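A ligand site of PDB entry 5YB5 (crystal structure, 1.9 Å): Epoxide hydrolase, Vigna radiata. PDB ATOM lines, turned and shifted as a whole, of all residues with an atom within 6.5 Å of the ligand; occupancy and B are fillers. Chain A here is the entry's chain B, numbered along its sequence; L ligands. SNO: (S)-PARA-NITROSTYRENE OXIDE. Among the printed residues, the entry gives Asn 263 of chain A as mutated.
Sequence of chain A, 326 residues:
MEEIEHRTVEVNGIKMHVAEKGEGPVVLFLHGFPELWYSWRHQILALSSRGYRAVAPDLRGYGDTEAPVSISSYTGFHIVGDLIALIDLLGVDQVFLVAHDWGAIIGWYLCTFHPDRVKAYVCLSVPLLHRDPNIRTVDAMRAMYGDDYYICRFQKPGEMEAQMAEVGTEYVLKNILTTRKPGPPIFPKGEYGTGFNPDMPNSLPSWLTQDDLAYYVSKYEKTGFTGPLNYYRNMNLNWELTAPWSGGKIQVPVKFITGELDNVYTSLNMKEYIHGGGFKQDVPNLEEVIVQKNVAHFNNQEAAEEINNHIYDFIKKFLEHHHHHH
OH of Tyr 232 is in hydrogen-bond range of O3 of the ligand, at 2.8 Å. O3 of the ligand lies within hydrogen-bond range of OH of Tyr 150 (2.8 Å).
The backbone carbonyl oxygen (O) of Pro 185 is in hydrogen-bond range of the backbone NH (N) of Tyr 150, 3.0 Å away. N of Phe 33 lies within hydrogen-bond range of OD2 of Asp 101 (2.9 Å). A ring nitrogen (NE2) of His 297 lies within hydrogen-bond range of the side-chain carboxylate of Asp 101, 3.0 Å away. The backbone carbonyl oxygen (O) of Phe 196 is in hydrogen-bond range of the side-chain hydroxyl (OG1) of Thr 179 (2.9 Å). The side-chain carboxylate (OD1) of Asp 262 lies within hydrogen-bond range of a ring nitrogen (ND1) of His 297 (2.5 Å). OG of Ser 125 lies close to ND1 of His 297, at 3.4 Å.
Residues that only touch the ligand: Asp 101, Phe 33, Asn 263, Phe 196, Ile 176, His 297 and Phe 298. Hydrophobic or aromatic side chains within 4 Å of the ligand: Phe 33, Tyr 150, Ile 176, Phe 196, Tyr 232, His 297 and Phe 298. Within 4 Å of the ligand: Phe 33, Asp 101, Tyr 150, Ile 176, Phe 196, Tyr 232, Asn 263, His 297 and Phe 298. The nearest printed residue that does not touch the ligand is Thr 179 (4.05 Å).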
ATOM      1  N   GLY A  32      -6.930  -4.582 -26.314  1.00  0.00           N
ATOM      2  CA  GLY A  32      -6.381  -5.261 -25.170  1.00  0.00           C
ATOM      3  C   GLY A  32      -5.613  -4.398 -24.193  1.00  0.00           C
ATOM      4  O   GLY A  32      -5.766  -3.220 -24.114  1.00  0.00           O
ATOM      5  N   PHE A  33      -4.742  -5.044 -23.447  1.00  0.00           N
ATOM      6  CA  PHE A  33      -3.947  -4.422 -22.436  1.00  0.00           C
ATOM      7  C   PHE A  33      -2.517  -4.205 -22.884  1.00  0.00           C
ATOM      8  O   PHE A  33      -1.926  -5.100 -23.409  1.00  0.00           O
ATOM      9  CB  PHE A  33      -3.976  -5.305 -21.194  1.00  0.00           C
ATOM     10  CG  PHE A  33      -3.078  -4.835 -20.096  1.00  0.00           C
ATOM     11  CD1 PHE A  33      -1.780  -5.230 -20.045  1.00  0.00           C
ATOM     12  CD2 PHE A  33      -3.515  -3.952 -19.167  1.00  0.00           C
ATOM     13  CE1 PHE A  33      -0.928  -4.786 -19.057  1.00  0.00           C
ATOM     14  CE2 PHE A  33      -2.658  -3.487 -18.183  1.00  0.00           C
ATOM     15  CZ  PHE A  33      -1.365  -3.903 -18.128  1.00  0.00           C
ATOM     16  N   PRO A  34      -1.923  -3.072 -22.567  1.00  0.00           N
ATOM     17  CA  PRO A  34      -2.554  -1.857 -22.090  1.00  0.00           C
ATOM     18  C   PRO A  34      -2.818  -0.850 -23.200  1.00  0.00           C
ATOM     19  O   PRO A  34      -2.153   0.129 -23.336  1.00  0.00           O
ATOM     20  CB  PRO A  34      -1.496  -1.326 -21.185  1.00  0.00           C
ATOM     21  CG  PRO A  34      -0.282  -1.601 -21.953  1.00  0.00           C
ATOM     22  CD  PRO A  34      -0.477  -2.912 -22.611  1.00  0.00           C
ATOM     23  N   ASP A 101      -5.877  -9.686 -27.622  1.00  0.00           N
ATOM     24  CA  ASP A 101      -5.442  -9.715 -26.225  1.00  0.00           C
ATOM     25  C   ASP A 101      -6.642  -9.815 -25.263  1.00  0.00           C
ATOM     26  O   ASP A 101      -7.513 -10.655 -25.472  1.00  0.00           O
ATOM     27  CB  ASP A 101      -4.573  -8.485 -25.944  1.00  0.00           C
ATOM     28  CG  ASP A 101      -3.838  -8.584 -24.654  1.00  0.00           C
ATOM     29  OD1 ASP A 101      -2.860  -9.360 -24.605  1.00  0.00           O
ATOM     30  OD2 ASP A 101      -4.228  -7.897 -23.694  1.00  0.00           O
ATOM     31  N   TRP A 102      -6.718  -8.993 -24.223  1.00  0.00           N
ATOM     32  CA  TRP A 102      -7.887  -9.056 -23.335  1.00  0.00           C
ATOM     33  C   TRP A 102      -9.196  -8.830 -24.087  1.00  0.00           C
ATOM     34  O   TRP A 102     -10.239  -9.410 -23.743  1.00  0.00           O
ATOM     35  CB  TRP A 102      -7.769  -8.024 -22.191  1.00  0.00           C
ATOM     36  CG  TRP A 102      -7.458  -8.690 -20.900  1.00  0.00           C
ATOM     37  CD1 TRP A 102      -6.281  -8.633 -20.211  1.00  0.00           C
ATOM     38  CD2 TRP A 102      -8.333  -9.532 -20.132  1.00  0.00           C
ATOM     39  NE1 TRP A 102      -6.360  -9.393 -19.084  1.00  0.00           N
ATOM     40  CE2 TRP A 102      -7.613  -9.958 -19.001  1.00  0.00           C
ATOM     41  CE3 TRP A 102      -9.645  -9.980 -20.308  1.00  0.00           C
ATOM     42  CZ2 TRP A 102      -8.174 -10.809 -18.031  1.00  0.00           C
ATOM     43  CZ3 TRP A 102     -10.206 -10.832 -19.337  1.00  0.00           C
ATOM     44  CH2 TRP A 102      -9.465 -11.237 -18.226  1.00  0.00           C
ATOM     45  N   ILE A 105     -10.235 -12.206 -25.215  1.00  0.00           N
ATOM     46  CA  ILE A 105     -10.830 -13.028 -24.165  1.00  0.00           C
ATOM     47  C   ILE A 105     -12.301 -12.638 -24.008  1.00  0.00           C
ATOM     48  O   ILE A 105     -13.185 -13.489 -23.912  1.00  0.00           O
ATOM     49  CB  ILE A 105     -10.094 -12.820 -22.826  1.00  0.00           C
ATOM     50  CG1 ILE A 105      -8.668 -13.409 -22.899  1.00  0.00           C
ATOM     51  CG2 ILE A 105     -10.866 -13.503 -21.714  1.00  0.00           C
ATOM     52  CD1 ILE A 105      -7.747 -12.928 -21.783  1.00  0.00           C
ATOM     53  N   SER A 125      -3.970 -12.883 -31.267  1.00  0.00           N
ATOM     54  CA  SER A 125      -3.156 -13.190 -30.106  1.00  0.00           C
ATOM     55  C   SER A 125      -3.639 -14.222 -29.117  1.00  0.00           C
ATOM     56  O   SER A 125      -2.977 -15.174 -28.886  1.00  0.00           O
ATOM     57  CB  SER A 125      -2.631 -11.939 -29.382  1.00  0.00           C
ATOM     58  OG  SER A 125      -2.031 -12.216 -28.169  1.00  0.00           O
ATOM     59  N   VAL A 126      -4.795 -14.014 -28.530  1.00  0.00           N
ATOM     60  CA  VAL A 126      -5.272 -14.903 -27.506  1.00  0.00           C
ATOM     61  C   VAL A 126      -6.351 -15.818 -27.954  1.00  0.00           C
ATOM     62  O   VAL A 126      -7.389 -15.378 -28.289  1.00  0.00           O
ATOM     63  CB  VAL A 126      -5.768 -14.127 -26.267  1.00  0.00           C
ATOM     64  CG1 VAL A 126      -6.120 -15.067 -25.161  1.00  0.00           C
ATOM     65  CG2 VAL A 126      -4.730 -13.173 -25.767  1.00  0.00           C
ATOM     66  N   TYR A 150       3.857 -12.387 -14.906  1.00  0.00           N
ATOM     67  CA  TYR A 150       3.234 -11.063 -14.858  1.00  0.00           C
ATOM     68  C   TYR A 150       1.797 -11.098 -14.378  1.00  0.00           C
ATOM     69  O   TYR A 150       1.382 -10.222 -13.615  1.00  0.00           O
ATOM     70  CB  TYR A 150       3.338 -10.305 -16.205  1.00  0.00           C
ATOM     71  CG  TYR A 150       2.467 -10.806 -17.318  1.00  0.00           C
ATOM     72  CD1 TYR A 150       2.677 -12.049 -17.900  1.00  0.00           C
ATOM     73  CD2 TYR A 150       1.427 -10.013 -17.825  1.00  0.00           C
ATOM     74  CE1 TYR A 150       1.899 -12.495 -18.912  1.00  0.00           C
ATOM     75  CE2 TYR A 150       0.642 -10.455 -18.853  1.00  0.00           C
ATOM     76  CZ  TYR A 150       0.885 -11.699 -19.398  1.00  0.00           C
ATOM     77  OH  TYR A 150       0.104 -12.159 -20.420  1.00  0.00           O
ATOM     78  N   ILE A 151       1.064 -12.098 -14.781  1.00  0.00           N
ATOM     79  CA  ILE A 151      -0.345 -12.208 -14.416  1.00  0.00           C
ATOM     80  C   ILE A 151      -0.497 -12.353 -12.913  1.00  0.00           C
ATOM     81  O   ILE A 151      -1.445 -11.890 -12.359  1.00  0.00           O
ATOM     82  CB  ILE A 151      -1.087 -13.276 -15.213  1.00  0.00           C
ATOM     83  CG1 ILE A 151      -1.238 -12.839 -16.661  1.00  0.00           C
ATOM     84  CG2 ILE A 151      -2.468 -13.445 -14.658  1.00  0.00           C
ATOM     85  CD1 ILE A 151      -1.942 -13.824 -17.529  1.00  0.00           C
ATOM     86  N   PHE A 154       0.090  -9.138 -11.254  1.00  0.00           N
ATOM     87  CA  PHE A 154      -1.044  -8.296 -11.479  1.00  0.00           C
ATOM     88  C   PHE A 154      -2.190  -8.441 -10.464  1.00  0.00           C
ATOM     89  O   PHE A 154      -2.963  -7.566 -10.324  1.00  0.00           O
ATOM     90  CB  PHE A 154      -1.548  -8.528 -12.897  1.00  0.00           C
ATOM     91  CG  PHE A 154      -0.752  -7.858 -13.931  1.00  0.00           C
ATOM     92  CD1 PHE A 154       0.458  -7.367 -13.650  1.00  0.00           C
ATOM     93  CD2 PHE A 154      -1.231  -7.754 -15.198  1.00  0.00           C
ATOM     94  CE1 PHE A 154       1.189  -6.755 -14.586  1.00  0.00           C
ATOM     95  CE2 PHE A 154      -0.517  -7.141 -16.152  1.00  0.00           C
ATOM     96  CZ  PHE A 154       0.713  -6.636 -15.845  1.00  0.00           C
ATOM     97  N   ILE A 176       6.434  -2.265 -22.697  1.00  0.00           N
ATOM     98  CA  ILE A 176       5.510  -3.314 -23.141  1.00  0.00           C
ATOM     99  C   ILE A 176       5.324  -3.361 -24.654  1.00  0.00           C
ATOM    100  O   ILE A 176       5.517  -4.409 -25.255  1.00  0.00           O
ATOM    101  CB  ILE A 176       4.134  -3.161 -22.462  1.00  0.00           C
ATOM    102  CG1 ILE A 176       4.249  -3.495 -20.975  1.00  0.00           C
ATOM    103  CG2 ILE A 176       3.086  -4.072 -23.119  1.00  0.00           C
ATOM    104  CD1 ILE A 176       3.144  -2.898 -20.097  1.00  0.00           C
ATOM    105  N   LEU A 177       4.963  -2.226 -25.239  1.00  0.00           N
ATOM    106  CA  LEU A 177       4.736  -2.120 -26.684  1.00  0.00           C
ATOM    107  C   LEU A 177       5.942  -2.602 -27.516  1.00  0.00           C
ATOM    108  O   LEU A 177       5.763  -3.290 -28.523  1.00  0.00           O
ATOM    109  CB  LEU A 177       4.375  -0.673 -27.046  1.00  0.00           C
ATOM    110  CG  LEU A 177       2.954  -0.242 -26.637  1.00  0.00           C
ATOM    111  CD1 LEU A 177       2.774   1.247 -26.740  1.00  0.00           C
ATOM    112  CD2 LEU A 177       1.878  -0.946 -27.431  1.00  0.00           C
ATOM    113  N   THR A 179       8.240  -4.816 -26.798  1.00  0.00           N
ATOM    114  CA  THR A 179       8.808  -6.128 -26.507  1.00  0.00           C
ATOM    115  C   THR A 179       8.749  -7.120 -27.704  1.00  0.00           C
ATOM    116  O   THR A 179       7.744  -7.208 -28.417  1.00  0.00           O
ATOM    117  CB  THR A 179       8.219  -6.764 -25.257  1.00  0.00           C
ATOM    118  OG1 THR A 179       9.061  -7.845 -24.859  1.00  0.00           O
ATOM    119  CG2 THR A 179       6.814  -7.292 -25.507  1.00  0.00           C
ATOM    120  N   PRO A 185       6.465 -13.569 -19.730  1.00  0.00           N
ATOM    121  CA  PRO A 185       6.991 -12.392 -19.033  1.00  0.00           C
ATOM    122  C   PRO A 185       7.086 -12.650 -17.527  1.00  0.00           C
ATOM    123  O   PRO A 185       6.050 -12.856 -16.873  1.00  0.00           O
ATOM    124  CB  PRO A 185       5.932 -11.318 -19.327  1.00  0.00           C
ATOM    125  CG  PRO A 185       5.293 -11.756 -20.617  1.00  0.00           C
ATOM    126  CD  PRO A 185       5.247 -13.249 -20.524  1.00  0.00           C
ATOM    127  N   PHE A 196       8.583  -6.384 -18.937  1.00  0.00           N
ATOM    128  CA  PHE A 196       8.380  -7.288 -20.090  1.00  0.00           C
ATOM    129  C   PHE A 196       9.520  -7.308 -21.112  1.00  0.00           C
ATOM    130  O   PHE A 196       9.528  -8.147 -22.022  1.00  0.00           O
ATOM    131  CB  PHE A 196       7.142  -6.851 -20.876  1.00  0.00           C
ATOM    132  CG  PHE A 196       5.846  -7.065 -20.156  1.00  0.00           C
ATOM    133  CD1 PHE A 196       5.368  -6.120 -19.269  1.00  0.00           C
ATOM    134  CD2 PHE A 196       5.079  -8.190 -20.421  1.00  0.00           C
ATOM    135  CE1 PHE A 196       4.150  -6.314 -18.644  1.00  0.00           C
ATOM    136  CE2 PHE A 196       3.866  -8.386 -19.772  1.00  0.00           C
ATOM    137  CZ  PHE A 196       3.404  -7.442 -18.901  1.00  0.00           C
ATOM    138  N   TYR A 232      -7.438  -8.742 -15.086  1.00  0.00           N
ATOM    139  CA  TYR A 232      -6.674  -9.927 -14.716  1.00  0.00           C
ATOM    140  C   TYR A 232      -7.081 -10.411 -13.332  1.00  0.00           C
ATOM    141  O   TYR A 232      -7.043 -11.607 -13.057  1.00  0.00           O
ATOM    142  CB  TYR A 232      -5.179  -9.607 -14.668  1.00  0.00           C
ATOM    143  CG  TYR A 232      -4.535  -9.253 -15.995  1.00  0.00           C
ATOM    144  CD1 TYR A 232      -3.974 -10.226 -16.799  1.00  0.00           C
ATOM    145  CD2 TYR A 232      -4.471  -7.922 -16.427  1.00  0.00           C
ATOM    146  CE1 TYR A 232      -3.361  -9.909 -17.987  1.00  0.00           C
ATOM    147  CE2 TYR A 232      -3.864  -7.594 -17.609  1.00  0.00           C
ATOM    148  CZ  TYR A 232      -3.313  -8.594 -18.388  1.00  0.00           C
ATOM    149  OH  TYR A 232      -2.699  -8.253 -19.570  1.00  0.00           O
ATOM    150  N   MET A 235      -9.810 -13.111 -13.344  1.00  0.00           N
ATOM    151  CA  MET A 235      -9.659 -14.358 -14.123  1.00  0.00           C
ATOM    152  C   MET A 235     -10.109 -15.606 -13.389  1.00  0.00           C
ATOM    153  O   MET A 235     -10.774 -16.453 -13.966  1.00  0.00           O
ATOM    154  CB  MET A 235      -8.213 -14.530 -14.649  1.00  0.00           C
ATOM    155  CG  MET A 235      -7.902 -13.635 -15.860  1.00  0.00           C
ATOM    156  SD  MET A 235      -6.121 -13.568 -16.169  1.00  0.00           S
ATOM    157  CE  MET A 235      -6.061 -14.464 -17.715  1.00  0.00           C
ATOM    158  N   ASP A 262       4.958 -13.468 -30.207  1.00  0.00           N
ATOM    159  CA  ASP A 262       4.032 -13.097 -29.161  1.00  0.00           C
ATOM    160  C   ASP A 262       4.339 -13.881 -27.900  1.00  0.00           C
ATOM    161  O   ASP A 262       4.466 -15.044 -27.949  1.00  0.00           O
ATOM    162  CB  ASP A 262       2.613 -13.459 -29.620  1.00  0.00           C
ATOM    163  CG  ASP A 262       1.527 -12.753 -28.816  1.00  0.00           C
ATOM    164  OD1 ASP A 262       1.720 -12.433 -27.628  1.00  0.00           O
ATOM    165  OD2 ASP A 262       0.486 -12.535 -29.396  1.00  0.00           O
ATOM    166  N   ASN A 263       4.415 -13.214 -26.752  1.00  0.00           N
ATOM    167  CA  ASN A 263       4.658 -13.940 -25.529  1.00  0.00           C
ATOM    168  C   ASN A 263       3.548 -14.937 -25.288  1.00  0.00           C
ATOM    169  O   ASN A 263       3.751 -15.919 -24.680  1.00  0.00           O
ATOM    170  CB  ASN A 263       4.744 -13.019 -24.338  1.00  0.00           C
ATOM    171  CG  ASN A 263       3.411 -12.515 -23.935  1.00  0.00           C
ATOM    172  OD1 ASN A 263       2.603 -13.204 -23.340  1.00  0.00           O
ATOM    173  ND2 ASN A 263       3.199 -11.311 -24.225  1.00  0.00           N
ATOM    174  N   VAL A 264       2.371 -14.666 -25.769  1.00  0.00           N
ATOM    175  CA  VAL A 264       1.271 -15.573 -25.557  1.00  0.00           C
ATOM    176  C   VAL A 264       1.484 -16.862 -26.345  1.00  0.00           C
ATOM    177  O   VAL A 264       1.374 -17.971 -25.797  1.00  0.00           O
ATOM    178  CB  VAL A 264      -0.097 -14.952 -25.953  1.00  0.00           C
ATOM    179  CG1 VAL A 264      -1.178 -15.983 -25.803  1.00  0.00           C
ATOM    180  CG2 VAL A 264      -0.394 -13.728 -25.104  1.00  0.00           C
ATOM    181  N   HIS A 297       3.755  -9.408 -30.350  1.00  0.00           N
ATOM    182  CA  HIS A 297       2.417  -9.376 -29.803  1.00  0.00           C
ATOM    183  C   HIS A 297       1.429  -8.396 -30.433  1.00  0.00           C
ATOM    184  O   HIS A 297       0.318  -8.746 -30.620  1.00  0.00           O
ATOM    185  CB  HIS A 297       2.474  -9.136 -28.299  1.00  0.00           C
ATOM    186  CG  HIS A 297       1.129  -9.130 -27.628  1.00  0.00           C
ATOM    187  ND1 HIS A 297       0.530 -10.269 -27.176  1.00  0.00           N
ATOM    188  CD2 HIS A 297       0.301  -8.115 -27.323  1.00  0.00           C
ATOM    189  CE1 HIS A 297      -0.624  -9.950 -26.614  1.00  0.00           C
ATOM    190  NE2 HIS A 297      -0.784  -8.658 -26.707  1.00  0.00           N
ATOM    191  N   PHE A 298       1.851  -7.196 -30.738  1.00  0.00           N
ATOM    192  CA  PHE A 298       0.959  -6.202 -31.234  1.00  0.00           C
ATOM    193  C   PHE A 298       0.810  -6.253 -32.720  1.00  0.00           C
ATOM    194  O   PHE A 298       0.993  -5.300 -33.368  1.00  0.00           O
ATOM    195  CB  PHE A 298       1.387  -4.845 -30.738  1.00  0.00           C
ATOM    196  CG  PHE A 298       1.498  -4.773 -29.260  1.00  0.00           C
ATOM    197  CD1 PHE A 298       2.638  -5.151 -28.647  1.00  0.00           C
ATOM    198  CD2 PHE A 298       0.437  -4.389 -28.501  1.00  0.00           C
ATOM    199  CE1 PHE A 298       2.743  -5.118 -27.284  1.00  0.00           C
ATOM    200  CE2 PHE A 298       0.533  -4.359 -27.140  1.00  0.00           C
ATOM    201  CZ  PHE A 298       1.683  -4.727 -26.537  1.00  0.00           C
HETATM  202  C1  SNO L   1       1.203  -8.255 -23.298  1.00  0.00           C
HETATM  203  C2  SNO L   1       1.170  -9.475 -22.945  1.00  0.00           C
HETATM  204  C3  SNO L   1       0.032 -10.017 -22.515  1.00  0.00           C
HETATM  205  C4  SNO L   1      -1.161  -9.248 -22.394  1.00  0.00           C
HETATM  206  C5  SNO L   1      -0.973  -7.865 -22.823  1.00  0.00           C
HETATM  207  C6  SNO L   1       0.248  -7.442 -23.248  1.00  0.00           C
HETATM  208  C7  SNO L   1      -2.437  -9.873 -21.855  1.00  0.00           C
HETATM  209  C8  SNO L   1      -2.541 -11.473 -21.848  1.00  0.00           C
HETATM  210  N1  SNO L   1       2.477  -7.854 -23.729  1.00  0.00           N
HETATM  211  O1  SNO L   1       2.855  -7.834 -24.861  1.00  0.00           O
HETATM  212  O2  SNO L   1       3.255  -7.549 -22.881  1.00  0.00           O
HETATM  213  O3  SNO L   1      -2.231 -10.686 -20.769  1.00  0.00           O
